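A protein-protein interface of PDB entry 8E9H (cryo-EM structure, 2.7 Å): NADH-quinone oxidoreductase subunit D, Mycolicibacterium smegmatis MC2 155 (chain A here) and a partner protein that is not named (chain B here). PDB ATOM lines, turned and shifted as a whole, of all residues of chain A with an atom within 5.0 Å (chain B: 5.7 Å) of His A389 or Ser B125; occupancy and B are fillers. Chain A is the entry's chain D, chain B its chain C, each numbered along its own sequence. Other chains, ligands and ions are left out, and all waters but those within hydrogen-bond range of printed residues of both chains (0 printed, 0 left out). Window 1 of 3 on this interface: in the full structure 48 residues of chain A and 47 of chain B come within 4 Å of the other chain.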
ATOM      1  N   GLN A 374       9.455 -31.468 -13.000  1.00  0.00           N
ATOM      2  CA  GLN A 374      10.560 -31.001 -12.179  1.00  0.00           C
ATOM      3  C   GLN A 374      11.849 -31.423 -12.859  1.00  0.00           C
ATOM      4  O   GLN A 374      12.105 -32.619 -13.007  1.00  0.00           O
ATOM      5  CB  GLN A 374      10.464 -31.596 -10.774  1.00  0.00           C
ATOM      6  CG  GLN A 374      11.608 -31.279  -9.846  1.00  0.00           C
ATOM      7  CD  GLN A 374      11.459 -31.994  -8.523  1.00  0.00           C
ATOM      8  OE1 GLN A 374      10.802 -33.029  -8.444  1.00  0.00           O
ATOM      9  NE2 GLN A 374      12.051 -31.442  -7.475  1.00  0.00           N
ATOM     10  N   VAL A 375      12.652 -30.451 -13.272  1.00  0.00           N
ATOM     11  CA  VAL A 375      13.811 -30.708 -14.113  1.00  0.00           C
ATOM     12  C   VAL A 375      15.011 -29.967 -13.552  1.00  0.00           C
ATOM     13  O   VAL A 375      14.869 -28.927 -12.903  1.00  0.00           O
ATOM     14  CB  VAL A 375      13.538 -30.290 -15.570  1.00  0.00           C
ATOM     15  CG1 VAL A 375      14.789 -30.379 -16.400  1.00  0.00           C
ATOM     16  CG2 VAL A 375      12.467 -31.175 -16.166  1.00  0.00           C
ATOM     17  N   TYR A 376      16.195 -30.521 -13.786  1.00  0.00           N
ATOM     18  CA  TYR A 376      17.455 -29.855 -13.494  1.00  0.00           C
ATOM     19  C   TYR A 376      18.283 -29.829 -14.767  1.00  0.00           C
ATOM     20  O   TYR A 376      18.573 -30.881 -15.342  1.00  0.00           O
ATOM     21  CB  TYR A 376      18.217 -30.560 -12.378  1.00  0.00           C
ATOM     22  CG  TYR A 376      19.301 -29.700 -11.792  1.00  0.00           C
ATOM     23  CD1 TYR A 376      20.551 -29.639 -12.382  1.00  0.00           C
ATOM     24  CD2 TYR A 376      19.070 -28.932 -10.668  1.00  0.00           C
ATOM     25  CE1 TYR A 376      21.545 -28.850 -11.860  1.00  0.00           C
ATOM     26  CE2 TYR A 376      20.056 -28.138 -10.139  1.00  0.00           C
ATOM     27  CZ  TYR A 376      21.292 -28.100 -10.738  1.00  0.00           C
ATOM     28  OH  TYR A 376      22.283 -27.308 -10.215  1.00  0.00           O
ATOM     29  N   GLY A 387      23.573 -24.119 -12.976  1.00  0.00           N
ATOM     30  CA  GLY A 387      22.491 -25.078 -12.909  1.00  0.00           C
ATOM     31  C   GLY A 387      21.166 -24.376 -12.694  1.00  0.00           C
ATOM     32  O   GLY A 387      21.106 -23.306 -12.105  1.00  0.00           O
ATOM     33  N   VAL A 388      20.099 -24.999 -13.171  1.00  0.00           N
ATOM     34  CA  VAL A 388      18.759 -24.454 -13.041  1.00  0.00           C
ATOM     35  C   VAL A 388      17.845 -25.592 -12.633  1.00  0.00           C
ATOM     36  O   VAL A 388      17.659 -26.545 -13.398  1.00  0.00           O
ATOM     37  CB  VAL A 388      18.271 -23.814 -14.348  1.00  0.00           C
ATOM     38  CG1 VAL A 388      16.835 -23.352 -14.207  1.00  0.00           C
ATOM     39  CG2 VAL A 388      19.184 -22.673 -14.740  1.00  0.00           C
ATOM     40  N   HIS A 389      17.302 -25.509 -11.428  1.00  0.00           N
ATOM     41  CA  HIS A 389      16.245 -26.402 -10.990  1.00  0.00           C
ATOM     42  C   HIS A 389      14.914 -25.705 -11.202  1.00  0.00           C
ATOM     43  O   HIS A 389      14.655 -24.658 -10.602  1.00  0.00           O
ATOM     44  CB  HIS A 389      16.403 -26.794  -9.526  1.00  0.00           C
ATOM     45  CG  HIS A 389      15.272 -27.621  -9.013  1.00  0.00           C
ATOM     46  ND1 HIS A 389      14.531 -27.261  -7.909  1.00  0.00           N
ATOM     47  CD2 HIS A 389      14.724 -28.766  -9.479  1.00  0.00           C
ATOM     48  CE1 HIS A 389      13.590 -28.164  -7.703  1.00  0.00           C
ATOM     49  NE2 HIS A 389      13.686 -29.088  -8.640  1.00  0.00           N
ATOM     50  N   MET A 390      14.080 -26.281 -12.057  1.00  0.00           N
ATOM     51  CA  MET A 390      12.848 -25.633 -12.459  1.00  0.00           C
ATOM     52  C   MET A 390      11.688 -26.595 -12.302  1.00  0.00           C
ATOM     53  O   MET A 390      11.758 -27.746 -12.742  1.00  0.00           O
ATOM     54  CB  MET A 390      12.935 -25.160 -13.898  1.00  0.00           C
ATOM     55  CG  MET A 390      11.735 -24.436 -14.364  1.00  0.00           C
ATOM     56  SD  MET A 390      12.041 -23.960 -16.054  1.00  0.00           S
ATOM     57  CE  MET A 390      11.920 -25.583 -16.777  1.00  0.00           C
ATOM     58  N   VAL A 391      10.622 -26.104 -11.687  1.00  0.00           N
ATOM     59  CA  VAL A 391       9.446 -26.890 -11.368  1.00  0.00           C
ATOM     60  C   VAL A 391       8.233 -26.179 -11.936  1.00  0.00           C
ATOM     61  O   VAL A 391       8.030 -24.983 -11.694  1.00  0.00           O
ATOM     62  CB  VAL A 391       9.294 -27.081  -9.849  1.00  0.00           C
ATOM     63  CG1 VAL A 391       8.184 -28.060  -9.555  1.00  0.00           C
ATOM     64  CG2 VAL A 391      10.603 -27.528  -9.246  1.00  0.00           C
ATOM     65  N   ARG A 400       8.518 -22.880  -9.660  1.00  0.00           N
ATOM     66  CA  ARG A 400       9.711 -22.618  -8.866  1.00  0.00           C
ATOM     67  C   ARG A 400      10.931 -22.659  -9.766  1.00  0.00           C
ATOM     68  O   ARG A 400      11.207 -23.689 -10.377  1.00  0.00           O
ATOM     69  CB  ARG A 400       9.844 -23.645  -7.738  1.00  0.00           C
ATOM     70  CG  ARG A 400      11.205 -23.690  -7.077  1.00  0.00           C
ATOM     71  CD  ARG A 400      11.562 -22.372  -6.447  1.00  0.00           C
ATOM     72  NE  ARG A 400      12.692 -22.508  -5.538  1.00  0.00           N
ATOM     73  CZ  ARG A 400      13.638 -21.595  -5.372  1.00  0.00           C
ATOM     74  NH1 ARG A 400      13.622 -20.452  -6.034  1.00  0.00           N
ATOM     75  NH2 ARG A 400      14.632 -21.838  -4.525  1.00  0.00           N
ATOM     76  N   VAL A 401      11.670 -21.560  -9.837  1.00  0.00           N
ATOM     77  CA  VAL A 401      12.908 -21.503 -10.602  1.00  0.00           C
ATOM     78  C   VAL A 401      14.034 -21.118  -9.660  1.00  0.00           C
ATOM     79  O   VAL A 401      13.973 -20.069  -9.010  1.00  0.00           O
ATOM     80  CB  VAL A 401      12.814 -20.512 -11.772  1.00  0.00           C
ATOM     81  CG1 VAL A 401      14.193 -20.229 -12.327  1.00  0.00           C
ATOM     82  CG2 VAL A 401      11.921 -21.069 -12.850  1.00  0.00           C
ATOM     83  N   HIS A 402      15.053 -21.965  -9.586  1.00  0.00           N
ATOM     84  CA  HIS A 402      16.218 -21.736  -8.752  1.00  0.00           C
ATOM     85  C   HIS A 402      17.469 -21.863  -9.604  1.00  0.00           C
ATOM     86  O   HIS A 402      17.614 -22.826 -10.361  1.00  0.00           O
ATOM     87  CB  HIS A 402      16.267 -22.741  -7.604  1.00  0.00           C
ATOM     88  CG  HIS A 402      17.480 -22.613  -6.742  1.00  0.00           C
ATOM     89  ND1 HIS A 402      18.592 -23.409  -6.904  1.00  0.00           N
ATOM     90  CD2 HIS A 402      17.752 -21.795  -5.699  1.00  0.00           C
ATOM     91  CE1 HIS A 402      19.503 -23.079  -6.007  1.00  0.00           C
ATOM     92  NE2 HIS A 402      19.017 -22.104  -5.261  1.00  0.00           N
ATOM     93  N   GLY B 123      24.545 -28.319  -4.994  1.00  0.00           N
ATOM     94  CA  GLY B 123      23.873 -27.366  -4.135  1.00  0.00           C
ATOM     95  C   GLY B 123      22.639 -27.988  -3.507  1.00  0.00           C
ATOM     96  O   GLY B 123      22.462 -29.201  -3.529  1.00  0.00           O
ATOM     97  N   VAL B 124      21.804 -27.120  -2.943  1.00  0.00           N
ATOM     98  CA  VAL B 124      20.548 -27.520  -2.323  1.00  0.00           C
ATOM     99  C   VAL B 124      19.517 -26.473  -2.712  1.00  0.00           C
ATOM    100  O   VAL B 124      19.691 -25.287  -2.412  1.00  0.00           O
ATOM    101  CB  VAL B 124      20.652 -27.627  -0.798  1.00  0.00           C
ATOM    102  CG1 VAL B 124      19.320 -28.050  -0.208  1.00  0.00           C
ATOM    103  CG2 VAL B 124      21.755 -28.581  -0.415  1.00  0.00           C
ATOM    104  N   SER B 125      18.453 -26.899  -3.376  1.00  0.00           N
ATOM    105  CA  SER B 125      17.402 -25.998  -3.823  1.00  0.00           C
ATOM    106  C   SER B 125      16.134 -26.285  -3.038  1.00  0.00           C
ATOM    107  O   SER B 125      15.694 -27.432  -2.963  1.00  0.00           O
ATOM    108  CB  SER B 125      17.143 -26.165  -5.319  1.00  0.00           C
ATOM    109  OG  SER B 125      18.356 -26.168  -6.047  1.00  0.00           O
ATOM    110  N   GLY B 126      15.555 -25.249  -2.456  1.00  0.00           N
ATOM    111  CA  GLY B 126      14.299 -25.395  -1.762  1.00  0.00           C
ATOM    112  C   GLY B 126      13.122 -25.115  -2.676  1.00  0.00           C
ATOM    113  O   GLY B 126      13.163 -24.223  -3.516  1.00  0.00           O
ATOM    114  N   VAL B 127      12.069 -25.909  -2.513  1.00  0.00           N
ATOM    115  CA  VAL B 127      10.800 -25.647  -3.179  1.00  0.00           C
ATOM    116  C   VAL B 127       9.689 -25.944  -2.187  1.00  0.00           C
ATOM    117  O   VAL B 127       9.839 -26.777  -1.292  1.00  0.00           O
ATOM    118  CB  VAL B 127      10.642 -26.467  -4.478  1.00  0.00           C
ATOM    119  CG1 VAL B 127      10.678 -27.937  -4.186  1.00  0.00           C
ATOM    120  CG2 VAL B 127       9.349 -26.100  -5.175  1.00  0.00           C
ATOM    121  N   HIS B 138      10.374 -29.252   0.088  1.00  0.00           N
ATOM    122  CA  HIS B 138      11.247 -30.191  -0.593  1.00  0.00           C
ATOM    123  C   HIS B 138      12.616 -29.559  -0.768  1.00  0.00           C
ATOM    124  O   HIS B 138      12.727 -28.377  -1.107  1.00  0.00           O
ATOM    125  CB  HIS B 138      10.699 -30.588  -1.962  1.00  0.00           C
ATOM    126  CG  HIS B 138       9.498 -31.476  -1.906  1.00  0.00           C
ATOM    127  ND1 HIS B 138       9.126 -32.282  -2.959  1.00  0.00           N
ATOM    128  CD2 HIS B 138       8.576 -31.675  -0.936  1.00  0.00           C
ATOM    129  CE1 HIS B 138       8.031 -32.945  -2.637  1.00  0.00           C
ATOM    130  NE2 HIS B 138       7.677 -32.595  -1.414  1.00  0.00           N
ATOM    131  N   ALA B 139      13.652 -30.351  -0.531  1.00  0.00           N
ATOM    132  CA  ALA B 139      15.027 -29.960  -0.786  1.00  0.00           C
ATOM    133  C   ALA B 139      15.581 -30.858  -1.877  1.00  0.00           C
ATOM    134  O   ALA B 139      15.440 -32.083  -1.808  1.00  0.00           O
ATOM    135  CB  ALA B 139      15.874 -30.069   0.481  1.00  0.00           C
ATOM    136  N   VAL B 140      16.200 -30.249  -2.880  1.00  0.00           N
ATOM    137  CA  VAL B 140      16.715 -30.956  -4.042  1.00  0.00           C
ATOM    138  C   VAL B 140      18.229 -30.826  -4.037  1.00  0.00           C
ATOM    139  O   VAL B 140      18.767 -29.715  -3.999  1.00  0.00           O
ATOM    140  CB  VAL B 140      16.116 -30.414  -5.346  1.00  0.00           C
ATOM    141  CG1 VAL B 140      16.661 -31.176  -6.535  1.00  0.00           C
ATOM    142  CG2 VAL B 140      14.610 -30.508  -5.298  1.00  0.00           C
ATOM    143  N   TYR B 141      18.908 -31.969  -4.081  1.00  0.00           N
ATOM    144  CA  TYR B 141      20.361 -32.065  -4.071  1.00  0.00           C
ATOM    145  C   TYR B 141      20.796 -32.571  -5.435  1.00  0.00           C
ATOM    146  O   TYR B 141      20.716 -33.776  -5.706  1.00  0.00           O
ATOM    147  CB  TYR B 141      20.829 -33.017  -2.970  1.00  0.00           C
ATOM    148  CG  TYR B 141      20.464 -32.578  -1.578  1.00  0.00           C
ATOM    149  CD1 TYR B 141      19.186 -32.767  -1.083  1.00  0.00           C
ATOM    150  CD2 TYR B 141      21.404 -32.000  -0.750  1.00  0.00           C
ATOM    151  CE1 TYR B 141      18.852 -32.372   0.190  1.00  0.00           C
ATOM    152  CE2 TYR B 141      21.081 -31.604   0.524  1.00  0.00           C
ATOM    153  CZ  TYR B 141      19.806 -31.793   0.990  1.00  0.00           C
ATOM    154  OH  TYR B 141      19.489 -31.397   2.265  1.00  0.00           O
ATOM    155  N   PRO B 142      21.220 -31.697  -6.345  1.00  0.00           N
ATOM    156  CA  PRO B 142      21.771 -32.168  -7.624  1.00  0.00           C
ATOM    157  C   PRO B 142      23.197 -32.662  -7.441  1.00  0.00           C
ATOM    158  O   PRO B 142      24.103 -31.878  -7.152  1.00  0.00           O
ATOM    159  CB  PRO B 142      21.708 -30.924  -8.512  1.00  0.00           C
ATOM    160  CG  PRO B 142      21.750 -29.792  -7.551  1.00  0.00           C
ATOM    161  CD  PRO B 142      20.999 -30.244  -6.350  1.00  0.00           C
ATOM    162  N   THR B 182      18.542 -21.952   1.596  1.00  0.00           N
ATOM    163  CA  THR B 182      17.218 -22.559   1.588  1.00  0.00           C
ATOM    164  C   THR B 182      16.520 -22.399   2.929  1.00  0.00           C
ATOM    165  O   THR B 182      15.293 -22.308   2.969  1.00  0.00           O
ATOM    166  CB  THR B 182      17.309 -24.031   1.209  1.00  0.00           C
ATOM    167  OG1 THR B 182      18.176 -24.706   2.122  1.00  0.00           O
ATOM    168  CG2 THR B 182      17.835 -24.184  -0.203  1.00  0.00           C
ATOM    169  N   PHE B 186      13.032 -20.557   2.858  1.00  0.00           N
ATOM    170  CA  PHE B 186      11.946 -21.490   3.126  1.00  0.00           C
ATOM    171  C   PHE B 186      11.800 -21.875   4.585  1.00  0.00           C
ATOM    172  O   PHE B 186      10.754 -22.420   4.950  1.00  0.00           O
ATOM    173  CB  PHE B 186      12.133 -22.771   2.307  1.00  0.00           C
ATOM    174  CG  PHE B 186      12.073 -22.550   0.833  1.00  0.00           C
ATOM    175  CD1 PHE B 186      10.863 -22.537   0.174  1.00  0.00           C
ATOM    176  CD2 PHE B 186      13.226 -22.348   0.105  1.00  0.00           C
ATOM    177  CE1 PHE B 186      10.804 -22.329  -1.180  1.00  0.00           C
ATOM    178  CE2 PHE B 186      13.172 -22.141  -1.250  1.00  0.00           C
ATOM    179  CZ  PHE B 186      11.959 -22.131  -1.893  1.00  0.00           C
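A ring nitrogen (ND1) of His A402 is in hydrogen-bond range of the side-chain hydroxyl of Ser B125.
The guanidinium group (NE) of Arg A400 is in hydrogen-bond range of the backbone carbonyl oxygen (O) of Gly B126 (2.7 Å).
Among the printed residues, merely in contact across the chains: Gln A374 with Val B140 (3.5 Å), Tyr A376 with Pro B142 (3.5 Å), His A389 with Ser B125 (3.8 Å), His A389 with Val B140 (3.5 Å), Arg A400 with Val B127 (3.6 Å) and Arg A400 with Phe B186 (3.6 Å).
Hydrophobic or aromatic side chains of chain A that line the printed part of chain B: Tyr A376, His A389 and His A402.
Among the printed residues, no Asp or Glu carboxylate lies within 4 Å of a Lys or Arg side-chain nitrogen of the other chain.
The backbone carbonyl oxygen (O) of Ser B125 sits at hydrogen-bond distance from the backbone NH (N) of Val B140 (2.9 Å).
The backbone NH of His B138 is in hydrogen-bond range of the backbone carbonyl oxygen of Val B127 (2.9 Å).
NE2 of His A389 lies within hydrogen-bond range of NE2 of Gln A374 (3.1 Å).
The backbone carbonyl oxygen of His A402 lies within hydrogen-bond range of the backbone NH of His A389 (2.9 Å).
N of Val A391 sits at hydrogen-bond distance from O of Arg A400.
His A389 touches two residues of chain B.
Val A391 touches none of the printed residues of chain B.
Of the printed residues of chain B, Arg A400 touches Gly B126 (2.7 Å), Val B127 (3.6 Å) and Phe B186 (3.6 Å).
Of the printed residues of chain A, Ser B125 touches His A389 (3.8 Å) and His A402 (2.9 Å).
Printed residues of chain A within 4 Å of Pro B142: Tyr A376 (3.5 Å).
The nearest residue of chain B that does not touch His A389 is Val B127 (4.6 Å).
The nearest residue of chain A that does not touch Ser B125 is Tyr A376 (4.8 Å).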
